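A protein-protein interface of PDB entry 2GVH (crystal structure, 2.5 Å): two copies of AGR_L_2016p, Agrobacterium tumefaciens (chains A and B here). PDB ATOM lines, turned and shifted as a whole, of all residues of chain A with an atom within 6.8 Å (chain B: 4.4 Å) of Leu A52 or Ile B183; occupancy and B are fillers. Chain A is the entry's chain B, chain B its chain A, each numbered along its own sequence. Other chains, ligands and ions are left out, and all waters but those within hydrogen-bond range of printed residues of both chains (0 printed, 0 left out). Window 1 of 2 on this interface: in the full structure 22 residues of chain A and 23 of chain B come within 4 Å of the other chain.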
ATOM      1  N   THR A  45      -1.117  -1.599  19.665  1.00  0.00           N
ATOM      2  CA  THR A  45      -1.017  -1.897  18.245  1.00  0.00           C
ATOM      3  C   THR A  45       0.068  -2.908  17.959  1.00  0.00           C
ATOM      4  O   THR A  45      -0.089  -3.760  17.088  1.00  0.00           O
ATOM      5  CB  THR A  45      -0.740  -0.641  17.387  1.00  0.00           C
ATOM      6  OG1 THR A  45       0.406   0.061  17.893  1.00  0.00           O
ATOM      7  CG2 THR A  45      -1.958   0.262  17.347  1.00  0.00           C
ATOM      8  N   LEU A  46       1.169  -2.808  18.690  1.00  0.00           N
ATOM      9  CA  LEU A  46       2.276  -3.724  18.496  1.00  0.00           C
ATOM     10  C   LEU A  46       1.951  -5.121  19.016  1.00  0.00           C
ATOM     11  O   LEU A  46       2.289  -6.107  18.383  1.00  0.00           O
ATOM     12  CB  LEU A  46       3.537  -3.183  19.147  1.00  0.00           C
ATOM     13  CG  LEU A  46       4.773  -3.933  18.679  1.00  0.00           C
ATOM     14  CD1 LEU A  46       5.810  -2.989  18.181  1.00  0.00           C
ATOM     15  CD2 LEU A  46       5.290  -4.743  19.821  1.00  0.00           C
ATOM     16  N   PHE A  47       1.312  -5.216  20.173  1.00  0.00           N
ATOM     17  CA  PHE A  47       0.785  -6.499  20.610  1.00  0.00           C
ATOM     18  C   PHE A  47      -0.628  -6.559  20.064  1.00  0.00           C
ATOM     19  O   PHE A  47      -1.641  -6.448  20.783  1.00  0.00           O
ATOM     20  CB  PHE A  47       0.855  -6.604  22.120  1.00  0.00           C
ATOM     21  CG  PHE A  47       2.246  -6.488  22.658  1.00  0.00           C
ATOM     22  CD1 PHE A  47       3.142  -7.529  22.509  1.00  0.00           C
ATOM     23  CD2 PHE A  47       2.660  -5.327  23.315  1.00  0.00           C
ATOM     24  CE1 PHE A  47       4.422  -7.433  22.995  1.00  0.00           C
ATOM     25  CE2 PHE A  47       3.934  -5.223  23.826  1.00  0.00           C
ATOM     26  CZ  PHE A  47       4.824  -6.286  23.655  1.00  0.00           C
ATOM     27  N   GLY A  48      -0.669  -6.696  18.747  1.00  0.00           N
ATOM     28  CA  GLY A  48      -1.867  -6.464  17.945  1.00  0.00           C
ATOM     29  C   GLY A  48      -1.375  -6.484  16.519  1.00  0.00           C
ATOM     30  O   GLY A  48      -0.345  -7.131  16.203  1.00  0.00           O
ATOM     31  N   GLY A  49      -2.081  -5.746  15.669  1.00  0.00           N
ATOM     32  CA  GLY A  49      -1.900  -5.823  14.222  1.00  0.00           C
ATOM     33  C   GLY A  49      -0.532  -5.370  13.757  1.00  0.00           C
ATOM     34  O   GLY A  49       0.045  -5.949  12.830  1.00  0.00           O
ATOM     35  N   THR A  50       0.000  -4.344  14.405  1.00  0.00           N
ATOM     36  CA  THR A  50       1.276  -3.848  14.008  1.00  0.00           C
ATOM     37  C   THR A  50       2.318  -4.906  14.258  1.00  0.00           C
ATOM     38  O   THR A  50       3.223  -5.122  13.399  1.00  0.00           O
ATOM     39  CB  THR A  50       1.624  -2.547  14.711  1.00  0.00           C
ATOM     40  OG1 THR A  50       0.611  -1.581  14.402  1.00  0.00           O
ATOM     41  CG2 THR A  50       2.941  -2.003  14.219  1.00  0.00           C
ATOM     42  N   GLY A  51       2.199  -5.581  15.401  1.00  0.00           N
ATOM     43  CA  GLY A  51       3.072  -6.714  15.696  1.00  0.00           C
ATOM     44  C   GLY A  51       3.077  -7.639  14.491  1.00  0.00           C
ATOM     45  O   GLY A  51       4.148  -8.100  14.033  1.00  0.00           O
ATOM     46  N   LEU A  52       1.885  -7.876  13.952  1.00  0.00           N
ATOM     47  CA  LEU A  52       1.761  -8.747  12.793  1.00  0.00           C
ATOM     48  C   LEU A  52       2.519  -8.190  11.612  1.00  0.00           C
ATOM     49  O   LEU A  52       3.338  -8.887  11.027  1.00  0.00           O
ATOM     50  CB  LEU A  52       0.304  -8.974  12.426  1.00  0.00           C
ATOM     51  CG  LEU A  52      -0.250 -10.140  13.217  1.00  0.00           C
ATOM     52  CD1 LEU A  52      -1.731 -10.288  13.004  1.00  0.00           C
ATOM     53  CD2 LEU A  52       0.473 -11.400  12.829  1.00  0.00           C
ATOM     54  N   ALA A  53       2.245  -6.938  11.269  1.00  0.00           N
ATOM     55  CA  ALA A  53       2.935  -6.264  10.165  1.00  0.00           C
ATOM     56  C   ALA A  53       4.474  -6.382  10.219  1.00  0.00           C
ATOM     57  O   ALA A  53       5.121  -6.624   9.213  1.00  0.00           O
ATOM     58  CB  ALA A  53       2.488  -4.784  10.113  1.00  0.00           C
ATOM     59  N   LEU A  54       5.046  -6.252  11.414  1.00  0.00           N
ATOM     60  CA  LEU A  54       6.486  -6.286  11.596  1.00  0.00           C
ATOM     61  C   LEU A  54       6.997  -7.666  11.399  1.00  0.00           C
ATOM     62  O   LEU A  54       8.069  -7.842  10.809  1.00  0.00           O
ATOM     63  CB  LEU A  54       6.922  -5.765  12.962  1.00  0.00           C
ATOM     64  CG  LEU A  54       6.835  -4.266  13.199  1.00  0.00           C
ATOM     65  CD1 LEU A  54       7.647  -3.799  14.395  1.00  0.00           C
ATOM     66  CD2 LEU A  54       7.322  -3.555  12.026  1.00  0.00           C
ATOM     67  N   MET A  55       6.243  -8.653  11.858  1.00  0.00           N
ATOM     68  CA  MET A  55       6.601 -10.032  11.556  1.00  0.00           C
ATOM     69  C   MET A  55       6.659 -10.256  10.041  1.00  0.00           C
ATOM     70  O   MET A  55       7.568 -10.901   9.535  1.00  0.00           O
ATOM     71  CB  MET A  55       5.628 -10.989  12.196  1.00  0.00           C
ATOM     72  CG  MET A  55       5.636 -10.948  13.714  1.00  0.00           C
ATOM     73  SD  MET A  55       4.308 -12.175  14.546  1.00  0.00           S
ATOM     74  CE  MET A  55       5.310 -13.788  14.351  1.00  0.00           C
ATOM     75  N   ASP A  56       5.702  -9.705   9.301  1.00  0.00           N
ATOM     76  CA  ASP A  56       5.744  -9.891   7.880  1.00  0.00           C
ATOM     77  C   ASP A  56       6.897  -9.097   7.291  1.00  0.00           C
ATOM     78  O   ASP A  56       7.605  -9.599   6.418  1.00  0.00           O
ATOM     79  CB  ASP A  56       4.390  -9.584   7.260  1.00  0.00           C
ATOM     80  CG  ASP A  56       4.444  -9.410   5.757  1.00  0.00           C
ATOM     81  OD1 ASP A  56       4.299 -10.412   5.029  1.00  0.00           O
ATOM     82  OD2 ASP A  56       4.593  -8.238   5.312  1.00  0.00           O
ATOM     83  N   ARG A  57       7.096  -7.850   7.767  1.00  0.00           N
ATOM     84  CA  ARG A  57       8.222  -7.049   7.199  1.00  0.00           C
ATOM     85  C   ARG A  57       9.574  -7.798   7.277  1.00  0.00           C
ATOM     86  O   ARG A  57      10.314  -7.885   6.289  1.00  0.00           O
ATOM     87  CB  ARG A  57       8.319  -5.673   7.818  1.00  0.00           C
ATOM     88  CG  ARG A  57       9.005  -4.612   6.914  1.00  0.00           C
ATOM     89  CD  ARG A  57       9.320  -3.309   7.681  1.00  0.00           C
ATOM     90  NE  ARG A  57       8.098  -2.741   8.179  1.00  0.00           N
ATOM     91  CZ  ARG A  57       7.984  -2.007   9.278  1.00  0.00           C
ATOM     92  NH1 ARG A  57       9.031  -1.723  10.040  1.00  0.00           N
ATOM     93  NH2 ARG A  57       6.790  -1.555   9.622  1.00  0.00           N
ATOM     94  N   THR A  73       3.706 -11.855  -0.102  1.00  0.00           N
ATOM     95  CA  THR A  73       3.249 -12.768   0.905  1.00  0.00           C
ATOM     96  C   THR A  73       2.036 -13.494   0.371  1.00  0.00           C
ATOM     97  O   THR A  73       0.971 -12.900   0.203  1.00  0.00           O
ATOM     98  CB  THR A  73       2.938 -12.033   2.154  1.00  0.00           C
ATOM     99  OG1 THR A  73       4.125 -11.377   2.577  1.00  0.00           O
ATOM    100  CG2 THR A  73       2.515 -12.983   3.231  1.00  0.00           C
ATOM    101  N   SER A  75       0.839 -16.269   1.840  1.00  0.00           N
ATOM    102  CA  SER A  75       0.047 -16.689   2.975  1.00  0.00           C
ATOM    103  C   SER A  75       0.771 -16.676   4.295  1.00  0.00           C
ATOM    104  O   SER A  75       2.002 -16.710   4.362  1.00  0.00           O
ATOM    105  CB  SER A  75      -0.556 -18.077   2.719  1.00  0.00           C
ATOM    106  OG  SER A  75       0.309 -19.055   3.184  1.00  0.00           O
ATOM    107  N   CYS A  76      -0.043 -16.688   5.335  1.00  0.00           N
ATOM    108  CA  CYS A  76       0.400 -16.508   6.693  1.00  0.00           C
ATOM    109  C   CYS A  76      -0.258 -17.583   7.575  1.00  0.00           C
ATOM    110  O   CYS A  76      -1.470 -17.629   7.674  1.00  0.00           O
ATOM    111  CB  CYS A  76      -0.070 -15.133   7.099  1.00  0.00           C
ATOM    112  SG  CYS A  76       0.340 -14.664   8.718  1.00  0.00           S
ATOM    113  N   ILE A  79      -1.408 -17.883  14.027  1.00  0.00           N
ATOM    114  CA  ILE A  79      -0.510 -17.328  15.031  1.00  0.00           C
ATOM    115  C   ILE A  79      -1.249 -17.178  16.362  1.00  0.00           C
ATOM    116  O   ILE A  79      -2.373 -16.669  16.391  1.00  0.00           O
ATOM    117  CB  ILE A  79       0.047 -15.955  14.573  1.00  0.00           C
ATOM    118  CG1 ILE A  79       0.890 -16.102  13.308  1.00  0.00           C
ATOM    119  CG2 ILE A  79       0.914 -15.321  15.654  1.00  0.00           C
ATOM    120  CD1 ILE A  79       1.087 -14.811  12.583  1.00  0.00           C
ATOM    121  N   PHE A  81      -1.173 -15.192  19.993  1.00  0.00           N
ATOM    122  CA  PHE A  81      -0.619 -14.008  20.628  1.00  0.00           C
ATOM    123  C   PHE A  81      -0.864 -13.995  22.104  1.00  0.00           C
ATOM    124  O   PHE A  81      -1.954 -14.358  22.561  1.00  0.00           O
ATOM    125  CB  PHE A  81      -1.287 -12.767  20.062  1.00  0.00           C
ATOM    126  CG  PHE A  81      -0.516 -12.121  18.986  1.00  0.00           C
ATOM    127  CD1 PHE A  81      -0.666 -12.546  17.677  1.00  0.00           C
ATOM    128  CD2 PHE A  81       0.371 -11.073  19.272  1.00  0.00           C
ATOM    129  CE1 PHE A  81       0.067 -11.936  16.657  1.00  0.00           C
ATOM    130  CE2 PHE A  81       1.109 -10.456  18.261  1.00  0.00           C
ATOM    131  CZ  PHE A  81       0.959 -10.887  16.959  1.00  0.00           C
ATOM    132  N   PHE A  93      12.166  -9.050  16.263  1.00  0.00           N
ATOM    133  CA  PHE A  93      11.579  -9.922  15.270  1.00  0.00           C
ATOM    134  C   PHE A  93      12.699 -10.603  14.477  1.00  0.00           C
ATOM    135  O   PHE A  93      13.504  -9.939  13.825  1.00  0.00           O
ATOM    136  CB  PHE A  93      10.675  -9.118  14.354  1.00  0.00           C
ATOM    137  CG  PHE A  93       9.579  -8.380  15.082  1.00  0.00           C
ATOM    138  CD1 PHE A  93       9.851  -7.220  15.785  1.00  0.00           C
ATOM    139  CD2 PHE A  93       8.279  -8.836  15.045  1.00  0.00           C
ATOM    140  CE1 PHE A  93       8.853  -6.537  16.460  1.00  0.00           C
ATOM    141  CE2 PHE A  93       7.275  -8.172  15.709  1.00  0.00           C
ATOM    142  CZ  PHE A  93       7.554  -6.999  16.423  1.00  0.00           C
ATOM    143  N   MET A 111       8.783 -13.569  17.416  1.00  0.00           N
ATOM    144  CA  MET A 111       8.597 -12.259  18.027  1.00  0.00           C
ATOM    145  C   MET A 111       8.799 -12.332  19.558  1.00  0.00           C
ATOM    146  O   MET A 111       7.951 -12.843  20.329  1.00  0.00           O
ATOM    147  CB  MET A 111       7.218 -11.696  17.699  1.00  0.00           C
ATOM    148  CG  MET A 111       6.834 -10.483  18.559  1.00  0.00           C
ATOM    149  SD  MET A 111       5.003  -9.811  18.202  1.00  0.00           S
ATOM    150  CE  MET A 111       4.881  -8.479  19.541  1.00  0.00           C
ATOM    151  N   PHE A 129       5.584 -17.815   7.454  1.00  0.00           N
ATOM    152  CA  PHE A 129       5.184 -17.042   6.290  1.00  0.00           C
ATOM    153  C   PHE A 129       5.582 -17.697   5.012  1.00  0.00           C
ATOM    154  O   PHE A 129       6.699 -18.176   4.876  1.00  0.00           O
ATOM    155  CB  PHE A 129       5.785 -15.658   6.351  1.00  0.00           C
ATOM    156  CG  PHE A 129       5.142 -14.785   7.355  1.00  0.00           C
ATOM    157  CD1 PHE A 129       5.486 -14.874   8.701  1.00  0.00           C
ATOM    158  CD2 PHE A 129       4.199 -13.846   6.960  1.00  0.00           C
ATOM    159  CE1 PHE A 129       4.874 -14.024   9.664  1.00  0.00           C
ATOM    160  CE2 PHE A 129       3.567 -12.985   7.914  1.00  0.00           C
ATOM    161  CZ  PHE A 129       3.900 -13.083   9.259  1.00  0.00           C
ATOM    162  N   GLY B 179       1.962  -7.457   2.665  1.00  0.00           N
ATOM    163  CA  GLY B 179       0.868  -8.266   3.177  1.00  0.00           C
ATOM    164  C   GLY B 179       0.678  -8.075   4.672  1.00  0.00           C
ATOM    165  O   GLY B 179      -0.434  -8.159   5.202  1.00  0.00           O
ATOM    166  N   GLY B 180       1.778  -7.828   5.366  1.00  0.00           N
ATOM    167  CA  GLY B 180       1.700  -7.569   6.804  1.00  0.00           C
ATOM    168  C   GLY B 180       0.822  -6.355   7.059  1.00  0.00           C
ATOM    169  O   GLY B 180       0.063  -6.304   8.024  1.00  0.00           O
ATOM    170  N   GLU B 181       0.905  -5.397   6.144  1.00  0.00           N
ATOM    171  CA  GLU B 181       0.209  -4.148   6.318  1.00  0.00           C
ATOM    172  C   GLU B 181      -1.246  -4.367   5.997  1.00  0.00           C
ATOM    173  O   GLU B 181      -2.140  -3.761   6.617  1.00  0.00           O
ATOM    174  CB  GLU B 181       0.811  -3.065   5.454  1.00  0.00           C
ATOM    175  CG  GLU B 181       0.784  -1.712   6.142  1.00  0.00           C
ATOM    176  CD  GLU B 181       1.887  -1.527   7.162  1.00  0.00           C
ATOM    177  OE1 GLU B 181       3.025  -1.997   6.937  1.00  0.00           O
ATOM    178  OE2 GLU B 181       1.619  -0.877   8.191  1.00  0.00           O
ATOM    179  N   ALA B 182      -1.497  -5.250   5.041  1.00  0.00           N
ATOM    180  CA  ALA B 182      -2.861  -5.654   4.808  1.00  0.00           C
ATOM    181  C   ALA B 182      -3.417  -6.369   6.057  1.00  0.00           C
ATOM    182  O   ALA B 182      -4.550  -6.123   6.483  1.00  0.00           O
ATOM    183  CB  ALA B 182      -2.933  -6.533   3.601  1.00  0.00           C
ATOM    184  N   ILE B 183      -2.628  -7.258   6.649  1.00  0.00           N
ATOM    185  CA  ILE B 183      -3.123  -8.019   7.769  1.00  0.00           C
ATOM    186  C   ILE B 183      -3.462  -7.082   8.919  1.00  0.00           C
ATOM    187  O   ILE B 183      -4.493  -7.205   9.565  1.00  0.00           O
ATOM    188  CB  ILE B 183      -2.122  -9.030   8.220  1.00  0.00           C
ATOM    189  CG1 ILE B 183      -2.073 -10.190   7.232  1.00  0.00           C
ATOM    190  CG2 ILE B 183      -2.538  -9.559   9.561  1.00  0.00           C
ATOM    191  CD1 ILE B 183      -0.851 -11.089   7.401  1.00  0.00           C
ATOM    192  N   ALA B 184      -2.587  -6.125   9.164  1.00  0.00           N
ATOM    193  CA  ALA B 184      -2.787  -5.204  10.243  1.00  0.00           C
ATOM    194  C   ALA B 184      -4.070  -4.421  10.090  1.00  0.00           C
ATOM    195  O   ALA B 184      -4.723  -4.095  11.104  1.00  0.00           O
ATOM    196  CB  ALA B 184      -1.600  -4.264  10.339  1.00  0.00           C
ATOM    197  N   TYR B 185      -4.431  -4.108   8.844  1.00  0.00           N
ATOM    198  CA  TYR B 185      -5.715  -3.411   8.605  1.00  0.00           C
ATOM    199  C   TYR B 185      -6.909  -4.309   8.944  1.00  0.00           C
ATOM    200  O   TYR B 185      -7.915  -3.855   9.495  1.00  0.00           O
ATOM    201  CB  TYR B 185      -5.828  -2.846   7.177  1.00  0.00           C
ATOM    202  CG  TYR B 185      -7.046  -1.977   6.978  1.00  0.00           C
ATOM    203  CD1 TYR B 185      -7.115  -0.705   7.543  1.00  0.00           C
ATOM    204  CD2 TYR B 185      -8.151  -2.433   6.234  1.00  0.00           C
ATOM    205  CE1 TYR B 185      -8.242   0.080   7.384  1.00  0.00           C
ATOM    206  CE2 TYR B 185      -9.284  -1.637   6.065  1.00  0.00           C
ATOM    207  CZ  TYR B 185      -9.319  -0.394   6.644  1.00  0.00           C
ATOM    208  OH  TYR B 185     -10.404   0.404   6.476  1.00  0.00           O
ATOM    209  N   MET B 186      -6.784  -5.588   8.627  1.00  0.00           N
ATOM    210  CA  MET B 186      -7.844  -6.529   8.903  1.00  0.00           C
ATOM    211  C   MET B 186      -8.026  -6.674  10.391  1.00  0.00           C
ATOM    212  O   MET B 186      -9.137  -6.818  10.878  1.00  0.00           O
ATOM    213  CB  MET B 186      -7.515  -7.873   8.298  1.00  0.00           C
ATOM    214  CG  MET B 186      -7.479  -7.841   6.791  1.00  0.00           C
ATOM    215  SD  MET B 186      -6.808  -9.510   6.116  1.00  0.00           S
ATOM    216  CE  MET B 186      -8.382 -10.602   6.200  1.00  0.00           C
ATOM    217  N   THR B 187      -6.914  -6.639  11.101  1.00  0.00           N
ATOM    218  CA  THR B 187      -6.910  -6.764  12.535  1.00  0.00           C
ATOM    219  C   THR B 187      -7.586  -5.556  13.119  1.00  0.00           C
ATOM    220  O   THR B 187      -8.420  -5.695  13.997  1.00  0.00           O
ATOM    221  CB  THR B 187      -5.457  -6.932  13.079  1.00  0.00           C
ATOM    222  OG1 THR B 187      -4.811  -8.001  12.375  1.00  0.00           O
ATOM    223  CG2 THR B 187      -5.472  -7.285  14.543  1.00  0.00           C
ATOM    224  N   LEU B 204      -6.099  -8.835  20.775  1.00  0.00           N
ATOM    225  CA  LEU B 204      -5.933  -9.943  19.851  1.00  0.00           C
ATOM    226  C   LEU B 204      -5.349 -11.142  20.600  1.00  0.00           C
ATOM    227  O   LEU B 204      -4.375 -10.961  21.303  1.00  0.00           O
ATOM    228  CB  LEU B 204      -4.957  -9.524  18.765  1.00  0.00           C
ATOM    229  CG  LEU B 204      -4.526 -10.621  17.796  1.00  0.00           C
ATOM    230  CD1 LEU B 204      -5.684 -11.008  16.931  1.00  0.00           C
ATOM    231  CD2 LEU B 204      -3.392 -10.109  16.937  1.00  0.00           C
ATOM    232  N   ILE B 210      -4.101 -17.036   6.818  1.00  0.00           N
ATOM    233  CA  ILE B 210      -4.589 -16.045   5.890  1.00  0.00           C
ATOM    234  C   ILE B 210      -3.875 -16.259   4.588  1.00  0.00           C
ATOM    235  O   ILE B 210      -2.653 -16.243   4.547  1.00  0.00           O
ATOM    236  CB  ILE B 210      -4.282 -14.614   6.387  1.00  0.00           C
ATOM    237  CG1 ILE B 210      -4.998 -14.349   7.710  1.00  0.00           C
ATOM    238  CG2 ILE B 210      -4.697 -13.581   5.349  1.00  0.00           C
ATOM    239  CD1 ILE B 210      -4.784 -12.956   8.265  1.00  0.00           C
ATOM    240  N   PHE B 212      -3.511 -14.857   0.604  1.00  0.00           N
ATOM    241  CA  PHE B 212      -3.689 -13.699  -0.255  1.00  0.00           C
ATOM    242  C   PHE B 212      -3.906 -14.093  -1.704  1.00  0.00           C
ATOM    243  O   PHE B 212      -3.093 -14.807  -2.288  1.00  0.00           O
ATOM    244  CB  PHE B 212      -2.466 -12.804  -0.162  1.00  0.00           C
ATOM    245  CG  PHE B 212      -2.370 -12.061   1.138  1.00  0.00           C
ATOM    246  CD1 PHE B 212      -3.123 -10.910   1.348  1.00  0.00           C
ATOM    247  CD2 PHE B 212      -1.554 -12.528   2.158  1.00  0.00           C
ATOM    248  CE1 PHE B 212      -3.055 -10.222   2.558  1.00  0.00           C
ATOM    249  CE2 PHE B 212      -1.481 -11.847   3.381  1.00  0.00           C
ATOM    250  CZ  PHE B 212      -2.229 -10.695   3.573  1.00  0.00           C
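The backbone carbonyl oxygen (O) of Ile B183 is in hydrogen-bond range of the side-chain hydroxyl (OG1) of Thr B187, 2.9 Å away. The side-chain carboxylate of Asp A56 is in hydrogen-bond range of the side-chain hydroxyl of Thr A73.
The backbone NH (N) of Gly B180 sits at hydrogen-bond distance from the side-chain carboxylate (OD2) of Asp A56 (2.8 Å). N of Cys A76 is in hydrogen-bond range of O of Ile B210 (2.8 Å).
No position is printed for both chains. Of the 12 pairs that touch across the chains among the printed residues, none has its exchanged pair printed and touching as well.
Printed residues of chain B within 4 Å of Leu A52: Ile B183 and Thr B187. Of the printed residues of chain A, Ile B183 touches Leu A52 (3.6 Å) and Cys A76 (3.99 Å). Printed residues of chain A within 4 Å of Leu B204: Phe A81 (3.7 Å). Printed residues of chain A within 4 Å of Gly B180: Ala A53 and Asp A56. Of the printed residues of chain B, Gly A49 touches Ala B184 and Thr B187. Printed residues of chain B within 4 Å of Ser A75: Ile B210 (3.2 Å).
Among the printed residues, pairs that only touch across the chains: Ser A75 with Ile B210 (3.2 Å), Thr A73 with Phe B212 (3.2 Å), Gly A49 with Ala B184 (3.4 Å), Ala A53 with Gly B180 (3.5 Å), Leu A52 with Ile B183 (3.6 Å), Phe A81 with Leu B204 (3.7 Å), Asp A56 with Gly B179 (3.8 Å), Gly A49 with Thr B187 (3.9 Å), Leu A52 with Thr B187 (3.9 Å) and Cys A76 with Ile B183 (3.99 Å).
Of the 21 printed residues of chain A, 8 touch a printed residue of chain B. Hydrophobic or aromatic side chains of chain A that line the printed part of chain B: Leu A52, Ala A53 and Phe A81. Of the 12 printed residues of chain B, 8 touch a printed residue of chain A. Among the printed residues, 12 pairs touch across the chains. Among the printed residues, no Asp or Glu carboxylate lies within 4 Å of a Lys or Arg side-chain nitrogen of the other chain.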
